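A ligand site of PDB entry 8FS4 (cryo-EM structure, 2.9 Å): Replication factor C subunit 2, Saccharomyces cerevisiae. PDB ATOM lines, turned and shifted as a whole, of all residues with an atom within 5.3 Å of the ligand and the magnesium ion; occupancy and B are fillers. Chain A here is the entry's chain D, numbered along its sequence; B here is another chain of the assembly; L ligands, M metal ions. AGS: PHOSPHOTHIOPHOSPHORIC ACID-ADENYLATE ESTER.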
ATOM      1  N   TRP A  27     -23.441  -8.432  15.581  1.00  0.00           N
ATOM      2  CA  TRP A  27     -24.474  -9.039  16.463  1.00  0.00           C
ATOM      3  C   TRP A  27     -24.920  -8.061  17.547  1.00  0.00           C
ATOM      4  O   TRP A  27     -26.018  -8.245  18.098  1.00  0.00           O
ATOM      5  CB  TRP A  27     -23.971 -10.349  17.084  1.00  0.00           C
ATOM      6  CG  TRP A  27     -23.681 -11.430  16.095  1.00  0.00           C
ATOM      7  CD1 TRP A  27     -23.767 -11.371  14.739  1.00  0.00           C
ATOM      8  CD2 TRP A  27     -23.257 -12.767  16.413  1.00  0.00           C
ATOM      9  NE1 TRP A  27     -23.415 -12.570  14.189  1.00  0.00           N
ATOM     10  CE2 TRP A  27     -23.099 -13.443  15.184  1.00  0.00           C
ATOM     11  CE3 TRP A  27     -22.995 -13.456  17.604  1.00  0.00           C
ATOM     12  CZ2 TRP A  27     -22.685 -14.779  15.115  1.00  0.00           C
ATOM     13  CZ3 TRP A  27     -22.589 -14.773  17.534  1.00  0.00           C
ATOM     14  CH2 TRP A  27     -22.440 -15.420  16.303  1.00  0.00           C
ATOM     15  N   VAL A  28     -24.082  -7.070  17.873  1.00  0.00           N
ATOM     16  CA  VAL A  28     -24.455  -6.039  18.888  1.00  0.00           C
ATOM     17  C   VAL A  28     -25.541  -5.136  18.293  1.00  0.00           C
ATOM     18  O   VAL A  28     -26.474  -4.780  19.036  1.00  0.00           O
ATOM     19  CB  VAL A  28     -23.221  -5.227  19.358  1.00  0.00           C
ATOM     20  CG1 VAL A  28     -22.368  -6.039  20.319  1.00  0.00           C
ATOM     21  CG2 VAL A  28     -22.393  -4.724  18.186  1.00  0.00           C
ATOM     22  N   GLU A  29     -25.443  -4.795  17.008  1.00  0.00           N
ATOM     23  CA  GLU A  29     -26.450  -3.921  16.353  1.00  0.00           C
ATOM     24  C   GLU A  29     -27.479  -4.793  15.642  1.00  0.00           C
ATOM     25  O   GLU A  29     -28.189  -4.276  14.763  1.00  0.00           O
ATOM     26  CB  GLU A  29     -25.754  -2.996  15.355  1.00  0.00           C
ATOM     27  CG  GLU A  29     -24.551  -2.292  15.958  1.00  0.00           C
ATOM     28  CD  GLU A  29     -23.642  -1.632  14.944  1.00  0.00           C
ATOM     29  OE1 GLU A  29     -23.952  -1.697  13.738  1.00  0.00           O
ATOM     30  OE2 GLU A  29     -22.602  -1.074  15.356  1.00  0.00           O
ATOM     31  N   TYR A  31     -28.838  -7.692  17.698  1.00  0.00           N
ATOM     32  CA  TYR A  31     -29.604  -8.249  18.845  1.00  0.00           C
ATOM     33  C   TYR A  31     -29.884  -7.142  19.857  1.00  0.00           C
ATOM     34  O   TYR A  31     -30.026  -7.453  21.049  1.00  0.00           O
ATOM     35  CB  TYR A  31     -28.874  -9.448  19.446  1.00  0.00           C
ATOM     36  CG  TYR A  31     -28.974 -10.700  18.612  1.00  0.00           C
ATOM     37  CD1 TYR A  31     -28.320 -10.804  17.391  1.00  0.00           C
ATOM     38  CD2 TYR A  31     -29.769 -11.764  19.014  1.00  0.00           C
ATOM     39  CE1 TYR A  31     -28.422 -11.946  16.612  1.00  0.00           C
ATOM     40  CE2 TYR A  31     -29.879 -12.908  18.242  1.00  0.00           C
ATOM     41  CZ  TYR A  31     -29.208 -13.005  17.044  1.00  0.00           C
ATOM     42  OH  TYR A  31     -29.321 -14.140  16.271  1.00  0.00           O
ATOM     43  N   ARG A  32     -29.946  -5.888  19.383  1.00  0.00           N
ATOM     44  CA  ARG A  32     -30.301  -4.775  20.256  1.00  0.00           C
ATOM     45  C   ARG A  32     -31.759  -4.925  20.685  1.00  0.00           C
ATOM     46  O   ARG A  32     -32.621  -5.120  19.827  1.00  0.00           O
ATOM     47  CB  ARG A  32     -30.091  -3.450  19.540  1.00  0.00           C
ATOM     48  CG  ARG A  32     -30.187  -2.243  20.440  1.00  0.00           C
ATOM     49  CD  ARG A  32     -30.027  -0.963  19.646  1.00  0.00           C
ATOM     50  NE  ARG A  32     -28.657  -0.460  19.712  1.00  0.00           N
ATOM     51  CZ  ARG A  32     -28.101   0.056  20.801  1.00  0.00           C
ATOM     52  NH1 ARG A  32     -28.761   0.143  21.943  1.00  0.00           N
ATOM     53  NH2 ARG A  32     -26.853   0.507  20.729  1.00  0.00           N
ATOM     54  N   PRO A  33     -32.075  -4.834  21.975  1.00  0.00           N
ATOM     55  CA  PRO A  33     -33.469  -4.993  22.399  1.00  0.00           C
ATOM     56  C   PRO A  33     -34.379  -3.981  21.719  1.00  0.00           C
ATOM     57  O   PRO A  33     -34.134  -2.774  21.753  1.00  0.00           O
ATOM     58  CB  PRO A  33     -33.404  -4.762  23.917  1.00  0.00           C
ATOM     59  CG  PRO A  33     -32.010  -5.059  24.287  1.00  0.00           C
ATOM     60  CD  PRO A  33     -31.182  -4.619  23.122  1.00  0.00           C
ATOM     61  N   GLU A  38     -37.050  -7.373  26.066  1.00  0.00           N
ATOM     62  CA  GLU A  38     -35.771  -7.936  25.639  1.00  0.00           C
ATOM     63  C   GLU A  38     -34.600  -7.401  26.434  1.00  0.00           C
ATOM     64  O   GLU A  38     -33.470  -7.833  26.199  1.00  0.00           O
ATOM     65  CB  GLU A  38     -35.563  -7.654  24.142  1.00  0.00           C
ATOM     66  CG  GLU A  38     -36.513  -8.426  23.240  1.00  0.00           C
ATOM     67  CD  GLU A  38     -36.259  -8.157  21.778  1.00  0.00           C
ATOM     68  OE1 GLU A  38     -35.211  -7.583  21.441  1.00  0.00           O
ATOM     69  OE2 GLU A  38     -37.121  -8.531  20.951  1.00  0.00           O
ATOM     70  N   VAL A  39     -34.825  -6.481  27.379  1.00  0.00           N
ATOM     71  CA  VAL A  39     -33.748  -5.895  28.174  1.00  0.00           C
ATOM     72  C   VAL A  39     -33.543  -6.792  29.397  1.00  0.00           C
ATOM     73  O   VAL A  39     -34.325  -6.774  30.331  1.00  0.00           O
ATOM     74  CB  VAL A  39     -34.067  -4.460  28.575  1.00  0.00           C
ATOM     75  CG1 VAL A  39     -33.088  -3.966  29.622  1.00  0.00           C
ATOM     76  CG2 VAL A  39     -34.034  -3.552  27.357  1.00  0.00           C
ATOM     77  N   THR A  40     -32.475  -7.584  29.359  1.00  0.00           N
ATOM     78  CA  THR A  40     -32.157  -8.560  30.399  1.00  0.00           C
ATOM     79  C   THR A  40     -31.490  -7.891  31.600  1.00  0.00           C
ATOM     80  O   THR A  40     -30.851  -6.840  31.491  1.00  0.00           O
ATOM     81  CB  THR A  40     -31.253  -9.648  29.837  1.00  0.00           C
ATOM     82  OG1 THR A  40     -31.922 -10.342  28.772  1.00  0.00           O
ATOM     83  CG2 THR A  40     -30.862 -10.649  30.908  1.00  0.00           C
ATOM     84  N   ALA A  41     -31.669  -8.525  32.757  1.00  0.00           N
ATOM     85  CA  ALA A  41     -30.878  -8.258  33.961  1.00  0.00           C
ATOM     86  C   ALA A  41     -31.230  -6.964  34.660  1.00  0.00           C
ATOM     87  O   ALA A  41     -30.747  -6.717  35.772  1.00  0.00           O
ATOM     88  CB  ALA A  41     -29.383  -8.238  33.611  1.00  0.00           C
ATOM     89  N   GLN A  42     -32.068  -6.134  34.051  1.00  0.00           N
ATOM     90  CA  GLN A  42     -32.477  -4.865  34.671  1.00  0.00           C
ATOM     91  C   GLN A  42     -33.989  -4.845  34.754  1.00  0.00           C
ATOM     92  O   GLN A  42     -34.678  -4.309  33.892  1.00  0.00           O
ATOM     93  CB  GLN A  42     -31.939  -3.684  33.881  1.00  0.00           C
ATOM     94  CG  GLN A  42     -30.490  -3.348  34.211  1.00  0.00           C
ATOM     95  CD  GLN A  42     -29.596  -3.302  32.999  1.00  0.00           C
ATOM     96  OE1 GLN A  42     -30.069  -3.239  31.869  1.00  0.00           O
ATOM     97  NE2 GLN A  42     -28.294  -3.334  33.223  1.00  0.00           N
ATOM     98  N   PRO A  66     -22.303   0.814  34.518  1.00  0.00           N
ATOM     99  CA  PRO A  66     -21.107   0.445  33.770  1.00  0.00           C
ATOM    100  C   PRO A  66     -21.378   0.439  32.276  1.00  0.00           C
ATOM    101  O   PRO A  66     -22.529   0.298  31.848  1.00  0.00           O
ATOM    102  CB  PRO A  66     -20.777  -0.955  34.290  1.00  0.00           C
ATOM    103  CG  PRO A  66     -21.472  -1.062  35.596  1.00  0.00           C
ATOM    104  CD  PRO A  66     -22.699  -0.231  35.468  1.00  0.00           C
ATOM    105  N   PRO A  67     -20.339   0.594  31.446  1.00  0.00           N
ATOM    106  CA  PRO A  67     -20.556   0.568  29.995  1.00  0.00           C
ATOM    107  C   PRO A  67     -21.124  -0.762  29.534  1.00  0.00           C
ATOM    108  O   PRO A  67     -20.864  -1.810  30.117  1.00  0.00           O
ATOM    109  CB  PRO A  67     -19.153   0.816  29.421  1.00  0.00           C
ATOM    110  CG  PRO A  67     -18.404   1.466  30.519  1.00  0.00           C
ATOM    111  CD  PRO A  67     -18.931   0.874  31.785  1.00  0.00           C
ATOM    112  N   GLY A  68     -21.924  -0.703  28.473  1.00  0.00           N
ATOM    113  CA  GLY A  68     -22.492  -1.903  27.880  1.00  0.00           C
ATOM    114  C   GLY A  68     -23.459  -2.634  28.781  1.00  0.00           C
ATOM    115  O   GLY A  68     -23.455  -3.876  28.797  1.00  0.00           O
ATOM    116  N   THR A  69     -24.278  -1.907  29.526  1.00  0.00           N
ATOM    117  CA  THR A  69     -25.253  -2.513  30.430  1.00  0.00           C
ATOM    118  C   THR A  69     -26.689  -2.409  29.937  1.00  0.00           C
ATOM    119  O   THR A  69     -27.566  -3.077  30.499  1.00  0.00           O
ATOM    120  CB  THR A  69     -25.161  -1.875  31.823  1.00  0.00           C
ATOM    121  OG1 THR A  69     -24.833  -0.481  31.686  1.00  0.00           O
ATOM    122  CG2 THR A  69     -24.101  -2.559  32.646  1.00  0.00           C
ATOM    123  N   GLY A  70     -26.952  -1.614  28.915  1.00  0.00           N
ATOM    124  CA  GLY A  70     -28.248  -1.555  28.285  1.00  0.00           C
ATOM    125  C   GLY A  70     -29.050  -0.285  28.486  1.00  0.00           C
ATOM    126  O   GLY A  70     -30.267  -0.315  28.311  1.00  0.00           O
ATOM    127  N   LYS A  71     -28.396   0.824  28.856  1.00  0.00           N
ATOM    128  CA  LYS A  71     -29.138   2.056  29.117  1.00  0.00           C
ATOM    129  C   LYS A  71     -29.719   2.635  27.834  1.00  0.00           C
ATOM    130  O   LYS A  71     -30.909   2.950  27.756  1.00  0.00           O
ATOM    131  CB  LYS A  71     -28.228   3.076  29.803  1.00  0.00           C
ATOM    132  CG  LYS A  71     -27.491   2.515  31.007  1.00  0.00           C
ATOM    133  CD  LYS A  71     -26.575   3.534  31.651  1.00  0.00           C
ATOM    134  CE  LYS A  71     -25.419   3.929  30.761  1.00  0.00           C
ATOM    135  NZ  LYS A  71     -24.459   2.813  30.600  1.00  0.00           N
ATOM    136  N   THR A  72     -28.881   2.789  26.805  1.00  0.00           N
ATOM    137  CA  THR A  72     -29.360   3.331  25.536  1.00  0.00           C
ATOM    138  C   THR A  72     -30.422   2.432  24.920  1.00  0.00           C
ATOM    139  O   THR A  72     -31.428   2.922  24.401  1.00  0.00           O
ATOM    140  CB  THR A  72     -28.193   3.512  24.581  1.00  0.00           C
ATOM    141  OG1 THR A  72     -27.184   4.328  25.198  1.00  0.00           O
ATOM    142  CG2 THR A  72     -28.641   4.160  23.307  1.00  0.00           C
ATOM    143  N   SER A  73     -30.213   1.116  24.966  1.00  0.00           N
ATOM    144  CA  SER A  73     -31.213   0.203  24.437  1.00  0.00           C
ATOM    145  C   SER A  73     -32.524   0.340  25.203  1.00  0.00           C
ATOM    146  O   SER A  73     -33.606   0.340  24.603  1.00  0.00           O
ATOM    147  CB  SER A  73     -30.700  -1.226  24.506  1.00  0.00           C
ATOM    148  OG  SER A  73     -30.307  -1.572  25.823  1.00  0.00           O
ATOM    149  N   ASP A 140     -27.824  11.810  25.952  1.00  0.00           N
ATOM    150  CA  ASP A 140     -26.905  10.715  26.156  1.00  0.00           C
ATOM    151  C   ASP A 140     -25.487  11.233  26.335  1.00  0.00           C
ATOM    152  O   ASP A 140     -25.114  12.276  25.797  1.00  0.00           O
ATOM    153  CB  ASP A 140     -26.963   9.743  24.973  1.00  0.00           C
ATOM    154  CG  ASP A 140     -26.551   8.331  25.363  1.00  0.00           C
ATOM    155  OD1 ASP A 140     -25.796   8.176  26.334  1.00  0.00           O
ATOM    156  OD2 ASP A 140     -26.978   7.377  24.678  1.00  0.00           O
ATOM    157  N   GLU A 141     -24.695  10.492  27.101  1.00  0.00           N
ATOM    158  CA  GLU A 141     -23.336  10.904  27.446  1.00  0.00           C
ATOM    159  C   GLU A 141     -23.344  12.295  28.083  1.00  0.00           C
ATOM    160  O   GLU A 141     -22.610  13.190  27.690  1.00  0.00           O
ATOM    161  CB  GLU A 141     -22.441  10.874  26.206  1.00  0.00           C
ATOM    162  CG  GLU A 141     -22.172   9.477  25.676  1.00  0.00           C
ATOM    163  CD  GLU A 141     -22.408   9.355  24.182  1.00  0.00           C
ATOM    164  OE1 GLU A 141     -22.075  10.307  23.447  1.00  0.00           O
ATOM    165  OE2 GLU A 141     -22.922   8.302  23.745  1.00  0.00           O
ATOM    166  N   ILE A 169     -28.301  10.124  30.279  1.00  0.00           N
ATOM    167  CA  ILE A 169     -27.551   8.877  30.233  1.00  0.00           C
ATOM    168  C   ILE A 169     -26.094   9.213  30.507  1.00  0.00           C
ATOM    169  O   ILE A 169     -25.526  10.107  29.877  1.00  0.00           O
ATOM    170  CB  ILE A 169     -27.703   8.158  28.883  1.00  0.00           C
ATOM    171  CG1 ILE A 169     -29.160   8.127  28.397  1.00  0.00           C
ATOM    172  CG2 ILE A 169     -27.105   6.760  28.970  1.00  0.00           C
ATOM    173  CD1 ILE A 169     -29.986   6.984  28.910  1.00  0.00           C
ATOM    174  N   CYS A 170     -25.493   8.491  31.453  1.00  0.00           N
ATOM    175  CA  CYS A 170     -24.100   8.724  31.806  1.00  0.00           C
ATOM    176  C   CYS A 170     -23.507   7.453  32.389  1.00  0.00           C
ATOM    177  O   CYS A 170     -24.234   6.552  32.805  1.00  0.00           O
ATOM    178  CB  CYS A 170     -23.957   9.885  32.804  1.00  0.00           C
ATOM    179  SG  CYS A 170     -24.698   9.548  34.407  1.00  0.00           S
ATOM    180  N   ASN A 171     -22.179   7.397  32.424  1.00  0.00           N
ATOM    181  CA  ASN A 171     -21.470   6.288  33.049  1.00  0.00           C
ATOM    182  C   ASN A 171     -20.975   6.612  34.447  1.00  0.00           C
ATOM    183  O   ASN A 171     -20.985   5.742  35.318  1.00  0.00           O
ATOM    184  CB  ASN A 171     -20.279   5.877  32.179  1.00  0.00           C
ATOM    185  CG  ASN A 171     -20.691   5.125  30.936  1.00  0.00           C
ATOM    186  OD1 ASN A 171     -20.382   5.533  29.822  1.00  0.00           O
ATOM    187  ND2 ASN A 171     -21.395   4.015  31.123  1.00  0.00           N
ATOM    188  N   LEU A 192     -23.639  -6.740  33.992  1.00  0.00           N
ATOM    189  CA  LEU A 192     -24.156  -7.984  33.415  1.00  0.00           C
ATOM    190  C   LEU A 192     -23.083  -9.060  33.555  1.00  0.00           C
ATOM    191  O   LEU A 192     -22.140  -9.117  32.772  1.00  0.00           O
ATOM    192  CB  LEU A 192     -24.566  -7.771  31.963  1.00  0.00           C
ATOM    193  CG  LEU A 192     -25.503  -6.589  31.719  1.00  0.00           C
ATOM    194  CD1 LEU A 192     -26.091  -6.638  30.325  1.00  0.00           C
ATOM    195  CD2 LEU A 192     -26.621  -6.578  32.742  1.00  0.00           C
ATOM    196  N   ARG A 200     -29.355 -14.560  27.890  1.00  0.00           N
ATOM    197  CA  ARG A 200     -29.340 -13.765  26.670  1.00  0.00           C
ATOM    198  C   ARG A 200     -28.249 -14.249  25.716  1.00  0.00           C
ATOM    199  O   ARG A 200     -28.492 -14.374  24.507  1.00  0.00           O
ATOM    200  CB  ARG A 200     -29.148 -12.291  26.999  1.00  0.00           C
ATOM    201  CG  ARG A 200     -29.158 -11.388  25.774  1.00  0.00           C
ATOM    202  CD  ARG A 200     -30.505 -11.415  25.082  1.00  0.00           C
ATOM    203  NE  ARG A 200     -30.608 -10.405  24.042  1.00  0.00           N
ATOM    204  CZ  ARG A 200     -31.657 -10.258  23.245  1.00  0.00           C
ATOM    205  NH1 ARG A 200     -32.717 -11.045  23.341  1.00  0.00           N
ATOM    206  NH2 ARG A 200     -31.648  -9.307  22.322  1.00  0.00           N
ATOM    207  N   LEU A 228     -22.072  -6.739  28.248  1.00  0.00           N
ATOM    208  CA  LEU A 228     -22.645  -7.697  27.315  1.00  0.00           C
ATOM    209  C   LEU A 228     -22.298  -7.362  25.879  1.00  0.00           C
ATOM    210  O   LEU A 228     -22.260  -8.257  25.022  1.00  0.00           O
ATOM    211  CB  LEU A 228     -24.157  -7.777  27.493  1.00  0.00           C
ATOM    212  CG  LEU A 228     -24.869  -8.997  26.895  1.00  0.00           C
ATOM    213  CD1 LEU A 228     -24.309 -10.292  27.446  1.00  0.00           C
ATOM    214  CD2 LEU A 228     -26.348  -8.910  27.175  1.00  0.00           C
ATOM    215  N   ARG A 229     -22.035  -6.086  25.585  1.00  0.00           N
ATOM    216  CA  ARG A 229     -21.607  -5.716  24.245  1.00  0.00           C
ATOM    217  C   ARG A 229     -20.328  -6.445  23.871  1.00  0.00           C
ATOM    218  O   ARG A 229     -20.210  -7.019  22.777  1.00  0.00           O
ATOM    219  CB  ARG A 229     -21.402  -4.212  24.161  1.00  0.00           C
ATOM    220  CG  ARG A 229     -20.940  -3.724  22.809  1.00  0.00           C
ATOM    221  CD  ARG A 229     -21.302  -2.270  22.626  1.00  0.00           C
ATOM    222  NE  ARG A 229     -20.988  -1.482  23.811  1.00  0.00           N
ATOM    223  CZ  ARG A 229     -21.385  -0.238  24.012  1.00  0.00           C
ATOM    224  NH1 ARG A 229     -22.139   0.402  23.125  1.00  0.00           N
ATOM    225  NH2 ARG A 229     -21.023   0.382  25.129  1.00  0.00           N
ATOM    226  N   ILE A 232     -20.775 -10.235  23.493  1.00  0.00           N
ATOM    227  CA  ILE A 232     -21.383 -10.602  22.216  1.00  0.00           C
ATOM    228  C   ILE A 232     -20.446 -10.379  21.042  1.00  0.00           C
ATOM    229  O   ILE A 232     -20.463 -11.173  20.090  1.00  0.00           O
ATOM    230  CB  ILE A 232     -22.721  -9.870  21.996  1.00  0.00           C
ATOM    231  CG1 ILE A 232     -23.793 -10.467  22.916  1.00  0.00           C
ATOM    232  CG2 ILE A 232     -23.163  -9.945  20.544  1.00  0.00           C
ATOM    233  CD1 ILE A 232     -25.005  -9.588  23.117  1.00  0.00           C
ATOM    234  N   ARG B 155     -18.386   7.543  20.380  1.00  0.00           N
ATOM    235  CA  ARG B 155     -19.192   6.465  20.960  1.00  0.00           C
ATOM    236  C   ARG B 155     -20.498   6.289  20.197  1.00  0.00           C
ATOM    237  O   ARG B 155     -20.959   5.153  19.990  1.00  0.00           O
ATOM    238  CB  ARG B 155     -19.461   6.756  22.431  1.00  0.00           C
ATOM    239  CG  ARG B 155     -18.207   6.823  23.267  1.00  0.00           C
ATOM    240  CD  ARG B 155     -18.494   7.284  24.682  1.00  0.00           C
ATOM    241  NE  ARG B 155     -19.671   6.648  25.245  1.00  0.00           N
ATOM    242  CZ  ARG B 155     -20.090   6.827  26.491  1.00  0.00           C
ATOM    243  NH1 ARG B 155     -19.439   7.605  27.338  1.00  0.00           N
ATOM    244  NH2 ARG B 155     -21.189   6.197  26.907  1.00  0.00           N
ATOM    245  N   ARG B 156     -21.126   7.388  19.783  1.00  0.00           N
ATOM    246  CA  ARG B 156     -22.380   7.328  19.047  1.00  0.00           C
ATOM    247  C   ARG B 156     -22.179   7.383  17.539  1.00  0.00           C
ATOM    248  O   ARG B 156     -23.013   6.864  16.790  1.00  0.00           O
ATOM    249  CB  ARG B 156     -23.314   8.469  19.461  1.00  0.00           C
ATOM    250  CG  ARG B 156     -24.145   8.249  20.735  1.00  0.00           C
ATOM    251  CD  ARG B 156     -24.535   6.797  20.986  1.00  0.00           C
ATOM    252  NE  ARG B 156     -25.351   6.263  19.912  1.00  0.00           N
ATOM    253  CZ  ARG B 156     -26.589   5.800  20.056  1.00  0.00           C
ATOM    254  NH1 ARG B 156     -27.210   5.837  21.212  1.00  0.00           N
ATOM    255  NH2 ARG B 156     -27.223   5.300  18.992  1.00  0.00           N
ATOM    256  N   GLU B 159     -21.633   3.812  16.444  1.00  0.00           N
ATOM    257  CA  GLU B 159     -22.658   2.882  16.904  1.00  0.00           C
ATOM    258  C   GLU B 159     -23.987   3.062  16.182  1.00  0.00           C
ATOM    259  O   GLU B 159     -24.698   2.080  15.951  1.00  0.00           O
ATOM    260  CB  GLU B 159     -22.888   3.051  18.411  1.00  0.00           C
ATOM    261  CG  GLU B 159     -23.684   1.927  19.050  1.00  0.00           C
ATOM    262  CD  GLU B 159     -23.849   2.108  20.545  1.00  0.00           C
ATOM    263  OE1 GLU B 159     -24.103   3.249  20.981  1.00  0.00           O
ATOM    264  OE2 GLU B 159     -23.744   1.099  21.277  1.00  0.00           O
ATOM    265  N   PRO B 180     -15.636   2.876  27.185  1.00  0.00           N
ATOM    266  CA  PRO B 180     -16.709   2.746  26.190  1.00  0.00           C
ATOM    267  C   PRO B 180     -16.215   2.507  24.770  1.00  0.00           C
ATOM    268  O   PRO B 180     -16.840   1.745  24.027  1.00  0.00           O
ATOM    269  CB  PRO B 180     -17.450   4.086  26.313  1.00  0.00           C
ATOM    270  CG  PRO B 180     -17.223   4.496  27.722  1.00  0.00           C
ATOM    271  CD  PRO B 180     -15.818   4.070  28.024  1.00  0.00           C
ATOM    272  N   ARG B 184     -16.999  -1.165  22.422  1.00  0.00           N
ATOM    273  CA  ARG B 184     -17.705  -1.268  21.156  1.00  0.00           C
ATOM    274  C   ARG B 184     -16.889  -1.923  20.060  1.00  0.00           C
ATOM    275  O   ARG B 184     -17.427  -2.177  18.976  1.00  0.00           O
ATOM    276  CB  ARG B 184     -18.141   0.119  20.678  1.00  0.00           C
ATOM    277  CG  ARG B 184     -19.158   0.796  21.567  1.00  0.00           C
ATOM    278  CD  ARG B 184     -19.164   2.288  21.332  1.00  0.00           C
ATOM    279  NE  ARG B 184     -20.425   2.897  21.732  1.00  0.00           N
ATOM    280  CZ  ARG B 184     -20.702   3.296  22.957  1.00  0.00           C
ATOM    281  NH1 ARG B 184     -19.842   3.159  23.950  1.00  0.00           N
ATOM    282  NH2 ARG B 184     -21.884   3.849  23.205  1.00  0.00           N
HETATM  283  PG  AGS L   1     -22.569   2.969  26.875  1.00  0.00           P
HETATM  284  S1G AGS L   1     -22.852   4.091  28.443  1.00  0.00           S
HETATM  285  O2G AGS L   1     -21.043   2.805  26.625  1.00  0.00           O
HETATM  286  O3G AGS L   1     -23.235   3.638  25.635  1.00  0.00           O
HETATM  287  PB  AGS L   1     -24.699   1.344  26.645  1.00  0.00           P
HETATM  288  O1B AGS L   1     -25.464   0.665  27.716  1.00  0.00           O
HETATM  289  O2B AGS L   1     -25.223   2.739  26.290  1.00  0.00           O
HETATM  290  O3B AGS L   1     -23.210   1.574  27.083  1.00  0.00           O
HETATM  291  PA  AGS L   1     -26.121  -0.157  24.841  1.00  0.00           P
HETATM  292  O1A AGS L   1     -27.122  -0.081  25.900  1.00  0.00           O
HETATM  293  O2A AGS L   1     -26.510   0.531  23.525  1.00  0.00           O
HETATM  294  O3A AGS L   1     -24.765   0.516  25.295  1.00  0.00           O
HETATM  295  O5' AGS L   1     -25.793  -1.673  24.600  1.00  0.00           O
HETATM  296  C5' AGS L   1     -24.867  -2.072  23.571  1.00  0.00           C
HETATM  297  C4' AGS L   1     -25.046  -3.538  23.295  1.00  0.00           C
HETATM  298  O4' AGS L   1     -25.294  -4.222  24.544  1.00  0.00           O
HETATM  299  C3' AGS L   1     -26.200  -3.884  22.363  1.00  0.00           C
HETATM  300  O3' AGS L   1     -25.797  -4.818  21.372  1.00  0.00           O
HETATM  301  C2' AGS L   1     -27.263  -4.487  23.291  1.00  0.00           C
HETATM  302  O2' AGS L   1     -27.979  -5.531  22.640  1.00  0.00           O
HETATM  303  C1' AGS L   1     -26.411  -5.065  24.419  1.00  0.00           C
HETATM  304  N9  AGS L   1     -27.084  -5.101  25.711  1.00  0.00           N
HETATM  305  C8  AGS L   1     -26.771  -4.362  26.812  1.00  0.00           C
HETATM  306  N7  AGS L   1     -27.530  -4.593  27.861  1.00  0.00           N
HETATM  307  C5  AGS L   1     -28.413  -5.557  27.392  1.00  0.00           C
HETATM  308  C6  AGS L   1     -29.488  -6.227  28.020  1.00  0.00           C
HETATM  309  N6  AGS L   1     -29.856  -6.028  29.286  1.00  0.00           N
HETATM  310  N1  AGS L   1     -30.170  -7.126  27.285  1.00  0.00           N
HETATM  311  C2  AGS L   1     -29.804  -7.337  26.011  1.00  0.00           C
HETATM  312  N3  AGS L   1     -28.815  -6.765  25.324  1.00  0.00           N
HETATM  313  C4  AGS L   1     -28.163  -5.875  26.083  1.00  0.00           C
HETATM  314 MG    MG M   1     -24.975   4.264  25.190  1.00  0.00          MG
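S1G of the ligand lies close to NH2 of Arg 155 of chain B, at 3.1 Å. The backbone carbonyl oxygen of Val 28 lies within hydrogen-bond range of an oxygen (O3') of the ligand, 2.4 Å away. S1G of the ligand sits close to ND2 of Asn 171 (3.1 Å). An oxygen (O1A) of the ligand sits at hydrogen-bond distance from the backbone NH of Thr 72. The backbone NH (N) of Thr 69 lies within hydrogen-bond range of an oxygen (O1B) of the ligand (3.4 Å). A nitrogen (N6) of the ligand is in hydrogen-bond range of the backbone carbonyl oxygen (O) of Thr 40 (2.6 Å). O3B of the ligand is in hydrogen-bond range of N of Gly 68, 3.0 Å away. An oxygen (O2') of the ligand sits at hydrogen-bond distance from the backbone carbonyl oxygen (O) of Tyr 31, at 3.2 Å. An oxygen (O1B) of the ligand lies within hydrogen-bond range of the backbone NH (N) of Gly 70, 3.0 Å away. The backbone NH (N) of Thr 40 is in hydrogen-bond range of a nitrogen (N1) of the ligand (3.1 Å). The backbone NH (N) of Ser 73 lies within hydrogen-bond range of an oxygen (O1A) of the ligand (3.4 Å). The guanidinium group (NH1) of Arg 184 of chain B lies within hydrogen-bond range of an oxygen (O2G) of the ligand (3.0 Å). NH1 of Arg 32 lies within salt-bridge range of O2A of the ligand (2.8 Å). The side-chain amino group (NZ) of Lys 71 is in salt-bridge range of an oxygen (O1B) of the ligand, 3.7 Å away. O2G of the ligand sits at hydrogen-bond distance from NH2 of Arg 229, at 2.8 Å. N of Lys 71 is in hydrogen-bond range of O1B of the ligand, at 3.1 Å.
The backbone carbonyl oxygen (O) of Pro 66 sits at hydrogen-bond distance from the side-chain amino group (NZ) of Lys 71 (3.4 Å). O of Pro 180 of chain B is in hydrogen-bond range of NH1 of Arg 184 of chain B, at 3.3 Å. The guanidinium group (NE) of Arg 155 of chain B is in salt-bridge range of the side-chain carboxylate (OE2) of Glu 141 (3.9 Å). The backbone carbonyl oxygen (O) of Tyr 31 lies within hydrogen-bond range of the guanidinium group (NH2) of Arg 200 (2.8 Å). NZ of Lys 71 lies close to ND2 of Asn 171. The backbone carbonyl oxygen of Gly 68 is in hydrogen-bond range of the backbone NH of Leu 228 (3.2 Å). The side-chain amide nitrogen (NE2) of Gln 42 lies within hydrogen-bond range of the backbone carbonyl oxygen (O) of Thr 69, at 2.8 Å. NH1 of Arg 229 is in salt-bridge range of OE2 of Glu 159 of chain B, 2.5 Å away.
CD of Pro 33 touches O2' of the ligand (3.4 Å). Glu 38 touches the ligand. C of Val 39 touches N6 of the ligand, at 3.8 Å. OE1 of Gln 42 touches N6 of the ligand, 3.8 Å away. Pro 67 touches the ligand (CB to O2G, 3.9 Å). Leu 192 touches the ligand (CD1 to N7, 3.5 Å). Arg 200 touches the ligand (NE to C2, 3.7 Å). CD2 of Leu 228 touches C4 of the ligand (3.7 Å). Glu 159 of chain B touches the ligand. Pro 180 of chain B touches the ligand (CB to O2G, 3.8 Å). Hydrophobic or aromatic side chains that line the ligand: Val 28, Pro 33, Val 39, Pro 67, Leu 192, Leu 228 and Pro 180 of chain B.
Asp 140 touches the magnesium ion. Arg 184 of chain B touches the magnesium ion (NH2 to MG, 3.7 Å). Of the 34 residues printed, 3 come within 4 Å of the magnesium ion. The nearest printed residue that does not touch the magnesium ion is Glu 159 of chain B (4.4 Å).
The magnesium ion is bound by O2B of the ligand (1.9 Å), O3G of the ligand (1.9 Å) and OG1 of Thr 72 (2.2 Å).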
